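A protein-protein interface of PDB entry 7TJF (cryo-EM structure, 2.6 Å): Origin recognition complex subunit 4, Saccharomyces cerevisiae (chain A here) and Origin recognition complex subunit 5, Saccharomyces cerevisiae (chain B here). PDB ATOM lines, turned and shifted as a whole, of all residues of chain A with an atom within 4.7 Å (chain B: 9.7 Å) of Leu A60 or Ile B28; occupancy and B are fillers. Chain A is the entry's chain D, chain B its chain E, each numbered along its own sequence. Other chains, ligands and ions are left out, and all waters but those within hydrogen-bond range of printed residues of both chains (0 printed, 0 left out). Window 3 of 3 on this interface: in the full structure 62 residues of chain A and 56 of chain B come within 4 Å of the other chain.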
ATOM      1  N   GLN A  56      22.749  16.154   8.385  1.00  0.00           N
ATOM      2  CA  GLN A  56      23.574  14.967   8.581  1.00  0.00           C
ATOM      3  C   GLN A  56      22.720  13.739   8.869  1.00  0.00           C
ATOM      4  O   GLN A  56      22.989  12.651   8.340  1.00  0.00           O
ATOM      5  CB  GLN A  56      24.562  15.222   9.718  1.00  0.00           C
ATOM      6  CG  GLN A  56      25.789  14.339   9.727  1.00  0.00           C
ATOM      7  CD  GLN A  56      26.720  14.675  10.874  1.00  0.00           C
ATOM      8  OE1 GLN A  56      26.299  15.244  11.881  1.00  0.00           O
ATOM      9  NE2 GLN A  56      27.993  14.328  10.726  1.00  0.00           N
ATOM     10  N   ARG A  57      21.673  13.906   9.691  1.00  0.00           N
ATOM     11  CA  ARG A  57      20.729  12.824   9.951  1.00  0.00           C
ATOM     12  C   ARG A  57      20.005  12.397   8.681  1.00  0.00           C
ATOM     13  O   ARG A  57      19.837  11.199   8.437  1.00  0.00           O
ATOM     14  CB  ARG A  57      19.721  13.254  11.015  1.00  0.00           C
ATOM     15  CG  ARG A  57      19.509  12.242  12.121  1.00  0.00           C
ATOM     16  CD  ARG A  57      19.076  12.921  13.404  1.00  0.00           C
ATOM     17  NE  ARG A  57      20.164  13.685  14.001  1.00  0.00           N
ATOM     18  CZ  ARG A  57      20.125  14.990  14.231  1.00  0.00           C
ATOM     19  NH1 ARG A  57      19.069  15.718  13.910  1.00  0.00           N
ATOM     20  NH2 ARG A  57      21.176  15.581  14.793  1.00  0.00           N
ATOM     21  N   ARG A  58      19.585  13.363   7.859  1.00  0.00           N
ATOM     22  CA  ARG A  58      18.900  13.043   6.609  1.00  0.00           C
ATOM     23  C   ARG A  58      19.818  12.305   5.643  1.00  0.00           C
ATOM     24  O   ARG A  58      19.393  11.346   4.988  1.00  0.00           O
ATOM     25  CB  ARG A  58      18.363  14.321   5.967  1.00  0.00           C
ATOM     26  CG  ARG A  58      17.649  14.106   4.646  1.00  0.00           C
ATOM     27  CD  ARG A  58      16.478  13.162   4.809  1.00  0.00           C
ATOM     28  NE  ARG A  58      15.954  12.709   3.527  1.00  0.00           N
ATOM     29  CZ  ARG A  58      14.681  12.792   3.168  1.00  0.00           C
ATOM     30  NH1 ARG A  58      13.769  13.310   3.974  1.00  0.00           N
ATOM     31  NH2 ARG A  58      14.312  12.336   1.975  1.00  0.00           N
ATOM     32  N   LEU A  59      21.084  12.727   5.560  1.00  0.00           N
ATOM     33  CA  LEU A  59      22.052  12.035   4.712  1.00  0.00           C
ATOM     34  C   LEU A  59      22.297  10.611   5.196  1.00  0.00           C
ATOM     35  O   LEU A  59      22.419   9.685   4.384  1.00  0.00           O
ATOM     36  CB  LEU A  59      23.363  12.821   4.665  1.00  0.00           C
ATOM     37  CG  LEU A  59      23.362  14.078   3.792  1.00  0.00           C
ATOM     38  CD1 LEU A  59      24.686  14.818   3.904  1.00  0.00           C
ATOM     39  CD2 LEU A  59      23.053  13.738   2.343  1.00  0.00           C
ATOM     40  N   LEU A  60      22.340  10.414   6.517  1.00  0.00           N
ATOM     41  CA  LEU A  60      22.540   9.071   7.053  1.00  0.00           C
ATOM     42  C   LEU A  60      21.329   8.171   6.806  1.00  0.00           C
ATOM     43  O   LEU A  60      21.496   6.996   6.461  1.00  0.00           O
ATOM     44  CB  LEU A  60      22.879   9.147   8.539  1.00  0.00           C
ATOM     45  CG  LEU A  60      24.304   9.598   8.874  1.00  0.00           C
ATOM     46  CD1 LEU A  60      24.563   9.500  10.365  1.00  0.00           C
ATOM     47  CD2 LEU A  60      25.345   8.807   8.093  1.00  0.00           C
ATOM     48  N   GLN A  61      20.102   8.694   6.957  1.00  0.00           N
ATOM     49  CA  GLN A  61      18.929   7.872   6.641  1.00  0.00           C
ATOM     50  C   GLN A  61      18.790   7.606   5.147  1.00  0.00           C
ATOM     51  O   GLN A  61      18.250   6.563   4.763  1.00  0.00           O
ATOM     52  CB  GLN A  61      17.629   8.484   7.177  1.00  0.00           C
ATOM     53  CG  GLN A  61      17.642   8.917   8.626  1.00  0.00           C
ATOM     54  CD  GLN A  61      16.446   9.775   8.993  1.00  0.00           C
ATOM     55  OE1 GLN A  61      15.377   9.661   8.395  1.00  0.00           O
ATOM     56  NE2 GLN A  61      16.623  10.645   9.980  1.00  0.00           N
ATOM     57  N   GLN A  62      19.252   8.522   4.294  1.00  0.00           N
ATOM     58  CA  GLN A  62      19.257   8.231   2.864  1.00  0.00           C
ATOM     59  C   GLN A  62      20.305   7.184   2.510  1.00  0.00           C
ATOM     60  O   GLN A  62      20.087   6.376   1.601  1.00  0.00           O
ATOM     61  CB  GLN A  62      19.486   9.507   2.055  1.00  0.00           C
ATOM     62  CG  GLN A  62      18.300  10.452   2.060  1.00  0.00           C
ATOM     63  CD  GLN A  62      18.416  11.568   1.046  1.00  0.00           C
ATOM     64  OE1 GLN A  62      17.471  12.327   0.839  1.00  0.00           O
ATOM     65  NE2 GLN A  62      19.573  11.676   0.406  1.00  0.00           N
ATOM     66  N   LEU A  63      21.436   7.173   3.218  1.00  0.00           N
ATOM     67  CA  LEU A  63      22.468   6.183   2.935  1.00  0.00           C
ATOM     68  C   LEU A  63      22.104   4.795   3.454  1.00  0.00           C
ATOM     69  O   LEU A  63      22.511   3.793   2.859  1.00  0.00           O
ATOM     70  CB  LEU A  63      23.804   6.636   3.521  1.00  0.00           C
ATOM     71  CG  LEU A  63      24.537   7.718   2.726  1.00  0.00           C
ATOM     72  CD1 LEU A  63      25.480   8.504   3.623  1.00  0.00           C
ATOM     73  CD2 LEU A  63      25.279   7.116   1.546  1.00  0.00           C
ATOM     74  N   TYR A  64      21.350   4.710   4.550  1.00  0.00           N
ATOM     75  CA  TYR A  64      20.911   3.426   5.082  1.00  0.00           C
ATOM     76  C   TYR A  64      19.584   2.955   4.497  1.00  0.00           C
ATOM     77  O   TYR A  64      19.173   1.825   4.775  1.00  0.00           O
ATOM     78  CB  TYR A  64      20.793   3.492   6.608  1.00  0.00           C
ATOM     79  CG  TYR A  64      22.111   3.369   7.337  1.00  0.00           C
ATOM     80  CD1 TYR A  64      22.777   2.152   7.415  1.00  0.00           C
ATOM     81  CD2 TYR A  64      22.690   4.474   7.946  1.00  0.00           C
ATOM     82  CE1 TYR A  64      23.980   2.042   8.080  1.00  0.00           C
ATOM     83  CE2 TYR A  64      23.890   4.376   8.609  1.00  0.00           C
ATOM     84  CZ  TYR A  64      24.531   3.158   8.675  1.00  0.00           C
ATOM     85  OH  TYR A  64      25.728   3.066   9.338  1.00  0.00           O
ATOM     86  N   ILE A 345      29.427   6.683   4.434  1.00  0.00           N
ATOM     87  CA  ILE A 345      28.730   6.881   5.717  1.00  0.00           C
ATOM     88  C   ILE A 345      29.600   7.495   6.816  1.00  0.00           C
ATOM     89  O   ILE A 345      29.168   8.495   7.420  1.00  0.00           O
ATOM     90  CB  ILE A 345      28.043   5.568   6.148  1.00  0.00           C
ATOM     91  CG1 ILE A 345      26.695   5.413   5.454  1.00  0.00           C
ATOM     92  CG2 ILE A 345      27.858   5.488   7.667  1.00  0.00           C
ATOM     93  CD1 ILE A 345      26.136   4.015   5.531  1.00  0.00           C
ATOM     94  N   VAL A 348      30.367  11.318   6.027  1.00  0.00           N
ATOM     95  CA  VAL A 348      29.302  12.231   6.430  1.00  0.00           C
ATOM     96  C   VAL A 348      29.211  12.309   7.949  1.00  0.00           C
ATOM     97  O   VAL A 348      29.102  13.399   8.522  1.00  0.00           O
ATOM     98  CB  VAL A 348      27.969  11.785   5.796  1.00  0.00           C
ATOM     99  CG1 VAL A 348      26.790  12.563   6.368  1.00  0.00           C
ATOM    100  CG2 VAL A 348      28.029  11.926   4.287  1.00  0.00           C
ATOM    101  N   ALA A 349      29.299  11.161   8.626  1.00  0.00           N
ATOM    102  CA  ALA A 349      29.024  11.107  10.056  1.00  0.00           C
ATOM    103  C   ALA A 349      30.143  11.684  10.919  1.00  0.00           C
ATOM    104  O   ALA A 349      29.881  12.046  12.071  1.00  0.00           O
ATOM    105  CB  ALA A 349      28.740   9.665  10.475  1.00  0.00           C
ATOM    106  N   ASN B   2      25.316  13.515  18.513  1.00  0.00           N
ATOM    107  CA  ASN B   2      24.542  13.111  19.681  1.00  0.00           C
ATOM    108  C   ASN B   2      25.256  12.021  20.466  1.00  0.00           C
ATOM    109  O   ASN B   2      24.664  11.382  21.333  1.00  0.00           O
ATOM    110  CB  ASN B   2      23.151  12.628  19.264  1.00  0.00           C
ATOM    111  CG  ASN B   2      22.323  13.720  18.619  1.00  0.00           C
ATOM    112  OD1 ASN B   2      21.966  13.634  17.445  1.00  0.00           O
ATOM    113  ND2 ASN B   2      22.014  14.759  19.387  1.00  0.00           N
ATOM    114  N   VAL B   3      26.535  11.808  20.159  1.00  0.00           N
ATOM    115  CA  VAL B   3      27.316  10.759  20.795  1.00  0.00           C
ATOM    116  C   VAL B   3      28.668  11.342  21.193  1.00  0.00           C
ATOM    117  O   VAL B   3      29.108  12.371  20.675  1.00  0.00           O
ATOM    118  CB  VAL B   3      27.470   9.523  19.871  1.00  0.00           C
ATOM    119  CG1 VAL B   3      28.660   9.654  18.917  1.00  0.00           C
ATOM    120  CG2 VAL B   3      27.510   8.237  20.673  1.00  0.00           C
ATOM    121  N   CYS B  17      35.248   5.884  13.845  1.00  0.00           N
ATOM    122  CA  CYS B  17      34.385   4.942  13.137  1.00  0.00           C
ATOM    123  C   CYS B  17      33.336   4.339  14.066  1.00  0.00           C
ATOM    124  O   CYS B  17      32.193   4.108  13.652  1.00  0.00           O
ATOM    125  CB  CYS B  17      35.222   3.844  12.487  1.00  0.00           C
ATOM    126  SG  CYS B  17      35.957   4.328  10.926  1.00  0.00           S
ATOM    127  N   LEU B  18      33.712   4.085  15.324  1.00  0.00           N
ATOM    128  CA  LEU B  18      32.760   3.604  16.320  1.00  0.00           C
ATOM    129  C   LEU B  18      31.673   4.637  16.591  1.00  0.00           C
ATOM    130  O   LEU B  18      30.498   4.285  16.741  1.00  0.00           O
ATOM    131  CB  LEU B  18      33.495   3.253  17.613  1.00  0.00           C
ATOM    132  CG  LEU B  18      33.731   1.777  17.932  1.00  0.00           C
ATOM    133  CD1 LEU B  18      34.229   1.023  16.718  1.00  0.00           C
ATOM    134  CD2 LEU B  18      34.711   1.639  19.082  1.00  0.00           C
ATOM    135  N   ALA B  19      32.050   5.915  16.654  1.00  0.00           N
ATOM    136  CA  ALA B  19      31.061   6.978  16.802  1.00  0.00           C
ATOM    137  C   ALA B  19      30.200   7.128  15.555  1.00  0.00           C
ATOM    138  O   ALA B  19      29.031   7.514  15.655  1.00  0.00           O
ATOM    139  CB  ALA B  19      31.756   8.298  17.125  1.00  0.00           C
ATOM    140  N   SER B  20      30.755   6.840  14.378  1.00  0.00           N
ATOM    141  CA  SER B  20      29.983   6.961  13.150  1.00  0.00           C
ATOM    142  C   SER B  20      29.006   5.806  12.960  1.00  0.00           C
ATOM    143  O   SER B  20      27.986   5.974  12.284  1.00  0.00           O
ATOM    144  CB  SER B  20      30.922   7.052  11.945  1.00  0.00           C
ATOM    145  OG  SER B  20      31.516   5.801  11.654  1.00  0.00           O
ATOM    146  N   TYR B  21      29.292   4.636  13.530  1.00  0.00           N
ATOM    147  CA  TYR B  21      28.447   3.467  13.307  1.00  0.00           C
ATOM    148  C   TYR B  21      27.510   3.154  14.468  1.00  0.00           C
ATOM    149  O   TYR B  21      26.362   2.772  14.236  1.00  0.00           O
ATOM    150  CB  TYR B  21      29.310   2.237  13.008  1.00  0.00           C
ATOM    151  CG  TYR B  21      29.935   2.254  11.633  1.00  0.00           C
ATOM    152  CD1 TYR B  21      29.175   2.541  10.506  1.00  0.00           C
ATOM    153  CD2 TYR B  21      31.288   1.984  11.462  1.00  0.00           C
ATOM    154  CE1 TYR B  21      29.746   2.556   9.246  1.00  0.00           C
ATOM    155  CE2 TYR B  21      31.866   1.997  10.212  1.00  0.00           C
ATOM    156  CZ  TYR B  21      31.093   2.286   9.109  1.00  0.00           C
ATOM    157  OH  TYR B  21      31.672   2.297   7.865  1.00  0.00           O
ATOM    158  N   ILE B  22      27.960   3.310  15.708  1.00  0.00           N
ATOM    159  CA  ILE B  22      27.183   2.916  16.879  1.00  0.00           C
ATOM    160  C   ILE B  22      26.424   4.129  17.394  1.00  0.00           C
ATOM    161  O   ILE B  22      27.032   5.121  17.813  1.00  0.00           O
ATOM    162  CB  ILE B  22      28.082   2.319  17.970  1.00  0.00           C
ATOM    163  CG1 ILE B  22      28.804   1.080  17.445  1.00  0.00           C
ATOM    164  CG2 ILE B  22      27.277   1.994  19.214  1.00  0.00           C
ATOM    165  CD1 ILE B  22      30.097   0.791  18.154  1.00  0.00           C
ATOM    166  N   SER B  23      25.095   4.044  17.376  1.00  0.00           N
ATOM    167  CA  SER B  23      24.239   5.159  17.755  1.00  0.00           C
ATOM    168  C   SER B  23      22.977   4.626  18.413  1.00  0.00           C
ATOM    169  O   SER B  23      22.562   3.490  18.176  1.00  0.00           O
ATOM    170  CB  SER B  23      23.875   6.025  16.543  1.00  0.00           C
ATOM    171  OG  SER B  23      23.067   7.123  16.924  1.00  0.00           O
ATOM    172  N   ALA B  24      22.353   5.474  19.229  1.00  0.00           N
ATOM    173  CA  ALA B  24      21.108   5.116  19.895  1.00  0.00           C
ATOM    174  C   ALA B  24      19.898   5.162  18.970  1.00  0.00           C
ATOM    175  O   ALA B  24      18.830   4.679  19.355  1.00  0.00           O
ATOM    176  CB  ALA B  24      20.866   6.034  21.095  1.00  0.00           C
ATOM    177  N   ASP B  25      20.035   5.728  17.773  1.00  0.00           N
ATOM    178  CA  ASP B  25      18.922   5.828  16.840  1.00  0.00           C
ATOM    179  C   ASP B  25      19.020   4.625  15.908  1.00  0.00           C
ATOM    180  O   ASP B  25      20.026   4.487  15.200  1.00  0.00           O
ATOM    181  CB  ASP B  25      19.006   7.162  16.081  1.00  0.00           C
ATOM    182  CG  ASP B  25      17.947   7.356  14.957  1.00  0.00           C
ATOM    183  OD1 ASP B  25      17.276   6.442  14.439  1.00  0.00           O
ATOM    184  OD2 ASP B  25      17.782   8.534  14.573  1.00  0.00           O
ATOM    185  N   PRO B  26      18.015   3.743  15.869  1.00  0.00           N
ATOM    186  CA  PRO B  26      18.126   2.524  15.051  1.00  0.00           C
ATOM    187  C   PRO B  26      18.020   2.755  13.553  1.00  0.00           C
ATOM    188  O   PRO B  26      18.333   1.836  12.787  1.00  0.00           O
ATOM    189  CB  PRO B  26      16.963   1.653  15.553  1.00  0.00           C
ATOM    190  CG  PRO B  26      16.513   2.279  16.836  1.00  0.00           C
ATOM    191  CD  PRO B  26      16.803   3.735  16.703  1.00  0.00           C
ATOM    192  N   ASP B  27      17.583   3.935  13.110  1.00  0.00           N
ATOM    193  CA  ASP B  27      17.458   4.192  11.681  1.00  0.00           C
ATOM    194  C   ASP B  27      18.812   4.430  11.025  1.00  0.00           C
ATOM    195  O   ASP B  27      18.976   4.144   9.835  1.00  0.00           O
ATOM    196  CB  ASP B  27      16.545   5.394  11.445  1.00  0.00           C
ATOM    197  CG  ASP B  27      15.237   5.013  10.797  1.00  0.00           C
ATOM    198  OD1 ASP B  27      14.882   3.815  10.831  1.00  0.00           O
ATOM    199  OD2 ASP B  27      14.559   5.912  10.254  1.00  0.00           O
ATOM    200  N   ILE B  28      19.783   4.938  11.777  1.00  0.00           N
ATOM    201  CA  ILE B  28      21.094   5.287  11.247  1.00  0.00           C
ATOM    202  C   ILE B  28      22.180   4.354  11.785  1.00  0.00           C
ATOM    203  O   ILE B  28      23.356   4.708  11.797  1.00  0.00           O
ATOM    204  CB  ILE B  28      21.425   6.761  11.528  1.00  0.00           C
ATOM    205  CG1 ILE B  28      21.420   7.041  13.031  1.00  0.00           C
ATOM    206  CG2 ILE B  28      20.406   7.655  10.864  1.00  0.00           C
ATOM    207  CD1 ILE B  28      21.995   8.392  13.399  1.00  0.00           C
ATOM    208  N   THR B  29      21.799   3.159  12.221  1.00  0.00           N
ATOM    209  CA  THR B  29      22.708   2.177  12.779  1.00  0.00           C
ATOM    210  C   THR B  29      22.676   0.918  11.925  1.00  0.00           C
ATOM    211  O   THR B  29      21.583   0.431  11.598  1.00  0.00           O
ATOM    212  CB  THR B  29      22.317   1.845  14.239  1.00  0.00           C
ATOM    213  OG1 THR B  29      22.337   3.043  15.022  1.00  0.00           O
ATOM    214  CG2 THR B  29      23.269   0.835  14.859  1.00  0.00           C
ATOM    215  N   PRO B  30      23.825   0.383  11.513  1.00  0.00           N
ATOM    216  CA  PRO B  30      23.823  -0.861  10.738  1.00  0.00           C
ATOM    217  C   PRO B  30      23.406  -2.049  11.594  1.00  0.00           C
ATOM    218  O   PRO B  30      23.503  -2.035  12.822  1.00  0.00           O
ATOM    219  CB  PRO B  30      25.276  -0.994  10.271  1.00  0.00           C
ATOM    220  CG  PRO B  30      26.059  -0.238  11.272  1.00  0.00           C
ATOM    221  CD  PRO B  30      25.190   0.893  11.733  1.00  0.00           C
ATOM    222  N   SER B  31      22.895  -3.078  10.914  1.00  0.00           N
ATOM    223  CA  SER B  31      22.488  -4.295  11.609  1.00  0.00           C
ATOM    224  C   SER B  31      23.691  -5.050  12.156  1.00  0.00           C
ATOM    225  O   SER B  31      23.664  -5.537  13.291  1.00  0.00           O
ATOM    226  CB  SER B  31      21.680  -5.189  10.670  1.00  0.00           C
ATOM    227  OG  SER B  31      20.471  -4.564  10.285  1.00  0.00           O
ATOM    228  N   LEU B  33      28.063  -5.006  12.591  1.00  0.00           N
ATOM    229  CA  LEU B  33      29.309  -4.255  12.595  1.00  0.00           C
ATOM    230  C   LEU B  33      30.432  -5.192  13.014  1.00  0.00           C
ATOM    231  O   LEU B  33      30.285  -5.933  13.991  1.00  0.00           O
ATOM    232  CB  LEU B  33      29.226  -3.059  13.547  1.00  0.00           C
ATOM    233  CG  LEU B  33      30.481  -2.199  13.694  1.00  0.00           C
ATOM    234  CD1 LEU B  33      30.791  -1.496  12.385  1.00  0.00           C
ATOM    235  CD2 LEU B  33      30.320  -1.200  14.827  1.00  0.00           C
ATOM    236  N   TYR B  50      34.487   3.337  24.507  1.00  0.00           N
ATOM    237  CA  TYR B  50      33.384   3.966  23.791  1.00  0.00           C
ATOM    238  C   TYR B  50      32.055   3.762  24.508  1.00  0.00           C
ATOM    239  O   TYR B  50      31.255   4.698  24.610  1.00  0.00           O
ATOM    240  CB  TYR B  50      33.308   3.420  22.367  1.00  0.00           C
ATOM    241  CG  TYR B  50      32.208   4.042  21.546  1.00  0.00           C
ATOM    242  CD1 TYR B  50      32.347   5.321  21.020  1.00  0.00           C
ATOM    243  CD2 TYR B  50      31.026   3.356  21.302  1.00  0.00           C
ATOM    244  CE1 TYR B  50      31.338   5.895  20.273  1.00  0.00           C
ATOM    245  CE2 TYR B  50      30.017   3.921  20.564  1.00  0.00           C
ATOM    246  CZ  TYR B  50      30.176   5.188  20.047  1.00  0.00           C
ATOM    247  OH  TYR B  50      29.163   5.738  19.304  1.00  0.00           O
ATOM    248  N   LYS B 125      11.943   4.138  19.741  1.00  0.00           N
ATOM    249  CA  LYS B 125      12.678   2.965  19.292  1.00  0.00           C
ATOM    250  C   LYS B 125      14.089   2.983  19.868  1.00  0.00           C
ATOM    251  O   LYS B 125      14.784   4.000  19.808  1.00  0.00           O
ATOM    252  CB  LYS B 125      12.730   2.933  17.767  1.00  0.00           C
ATOM    253  CG  LYS B 125      11.719   2.008  17.120  1.00  0.00           C
ATOM    254  CD  LYS B 125      11.468   2.414  15.675  1.00  0.00           C
ATOM    255  CE  LYS B 125      11.222   1.209  14.788  1.00  0.00           C
ATOM    256  NZ  LYS B 125      11.939   1.322  13.490  1.00  0.00           N
ATOM    257  N   CYS B 127      17.956   0.718  20.748  1.00  0.00           N
ATOM    258  CA  CYS B 127      18.928  -0.226  20.219  1.00  0.00           C
ATOM    259  C   CYS B 127      19.397  -1.155  21.327  1.00  0.00           C
ATOM    260  O   CYS B 127      19.690  -0.712  22.441  1.00  0.00           O
ATOM    261  CB  CYS B 127      20.139   0.489  19.611  1.00  0.00           C
ATOM    262  SG  CYS B 127      19.892   1.174  17.967  1.00  0.00           S
ATOM    263  N   PHE B 129      22.554  -3.553  21.711  1.00  0.00           N
ATOM    264  CA  PHE B 129      23.841  -3.892  21.118  1.00  0.00           C
ATOM    265  C   PHE B 129      24.325  -5.212  21.705  1.00  0.00           C
ATOM    266  O   PHE B 129      24.656  -5.293  22.890  1.00  0.00           O
ATOM    267  CB  PHE B 129      24.851  -2.770  21.340  1.00  0.00           C
ATOM    268  CG  PHE B 129      24.538  -1.534  20.556  1.00  0.00           C
ATOM    269  CD1 PHE B 129      24.789  -1.486  19.194  1.00  0.00           C
ATOM    270  CD2 PHE B 129      23.967  -0.434  21.170  1.00  0.00           C
ATOM    271  CE1 PHE B 129      24.491  -0.353  18.462  1.00  0.00           C
ATOM    272  CE2 PHE B 129      23.667   0.699  20.445  1.00  0.00           C
ATOM    273  CZ  PHE B 129      23.924   0.736  19.088  1.00  0.00           C
ATOM    274  N   ASN B 163      15.156  -3.069  18.735  1.00  0.00           N
ATOM    275  CA  ASN B 163      15.880  -3.583  17.582  1.00  0.00           C
ATOM    276  C   ASN B 163      17.254  -4.049  18.035  1.00  0.00           C
ATOM    277  O   ASN B 163      17.969  -3.312  18.720  1.00  0.00           O
ATOM    278  CB  ASN B 163      15.995  -2.515  16.494  1.00  0.00           C
ATOM    279  CG  ASN B 163      14.656  -1.891  16.151  1.00  0.00           C
ATOM    280  OD1 ASN B 163      14.276  -0.862  16.707  1.00  0.00           O
ATOM    281  ND2 ASN B 163      13.928  -2.518  15.235  1.00  0.00           N
ATOM    282  N   LYS B 165      21.087  -4.998  17.539  1.00  0.00           N
ATOM    283  CA  LYS B 165      22.235  -4.664  16.710  1.00  0.00           C
ATOM    284  C   LYS B 165      23.399  -5.550  17.119  1.00  0.00           C
ATOM    285  O   LYS B 165      23.680  -5.699  18.311  1.00  0.00           O
ATOM    286  CB  LYS B 165      22.613  -3.187  16.850  1.00  0.00           C
ATOM    287  CG  LYS B 165      21.497  -2.224  16.511  1.00  0.00           C
ATOM    288  CD  LYS B 165      20.992  -2.440  15.097  1.00  0.00           C
ATOM    289  CE  LYS B 165      19.968  -1.387  14.717  1.00  0.00           C
ATOM    290  NZ  LYS B 165      19.743  -1.334  13.249  1.00  0.00           N
ATOM    291  N   PRO B 185      29.943  -3.316   7.361  1.00  0.00           N
ATOM    292  CA  PRO B 185      30.940  -2.331   7.805  1.00  0.00           C
ATOM    293  C   PRO B 185      31.923  -2.924   8.808  1.00  0.00           C
ATOM    294  O   PRO B 185      31.536  -3.531   9.813  1.00  0.00           O
ATOM    295  CB  PRO B 185      30.090  -1.216   8.433  1.00  0.00           C
ATOM    296  CG  PRO B 185      28.719  -1.784   8.580  1.00  0.00           C
ATOM    297  CD  PRO B 185      28.567  -2.821   7.526  1.00  0.00           C
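Printed residues of chain A that touch a printed residue of chain B: Arg A57, Leu A60, Gln A61, Tyr A64, Ile A345 and Ala A349.
Hydrophobic or aromatic side chains of chain B that line the printed part of chain A: Tyr B21, Ile B28 and Pro B30.
Among the printed residues, 9 pairs touch across the chains.
Among the printed residues, no Asp or Glu carboxylate lies within 4 Å of a Lys or Arg side-chain nitrogen of the other chain.
Among the printed residues, pairs that only touch across the chains: Tyr A64 with Ile B28, Tyr A64 with Pro B30, Tyr A64 with Tyr B21, Leu A60 with Ile B28, Ala A349 with Ser B20, Tyr A64 with Asp B27, Gln A61 with Ile B28 and Ile A345 with Tyr B21.
O of Ala A349 is in hydrogen-bond range of NE2 of Gln A56 (3.3 Å).
OG of Ser B20 lies within hydrogen-bond range of O of Cys B17 (2.7 Å).
OD1 of Asp B25 lies within hydrogen-bond range of N of Asp B27, at 2.9 Å.
No residue of chain B comes within 4 Å of Leu A59.
Leu A60 touches one residue of chain B.
Printed residues of chain B within 4 Å of Ala A349: Ser B20 (3.7 Å).
Asp B25 touches none of the printed residues of chain A.
Of the printed residues of chain A, Asp B27 touches Tyr A64 (3.8 Å).
Of the printed residues of chain A, Ile B28 touches Leu A60, Gln A61 and Tyr A64.
Cys B127 touches none of the printed residues of chain A.
The nearest residue of chain A that does not touch Ile B28 is Arg A57 (4.3 Å).
OD1 of Asn B2 sits at hydrogen-bond distance from NH2 of Arg A57 (3.4 Å).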
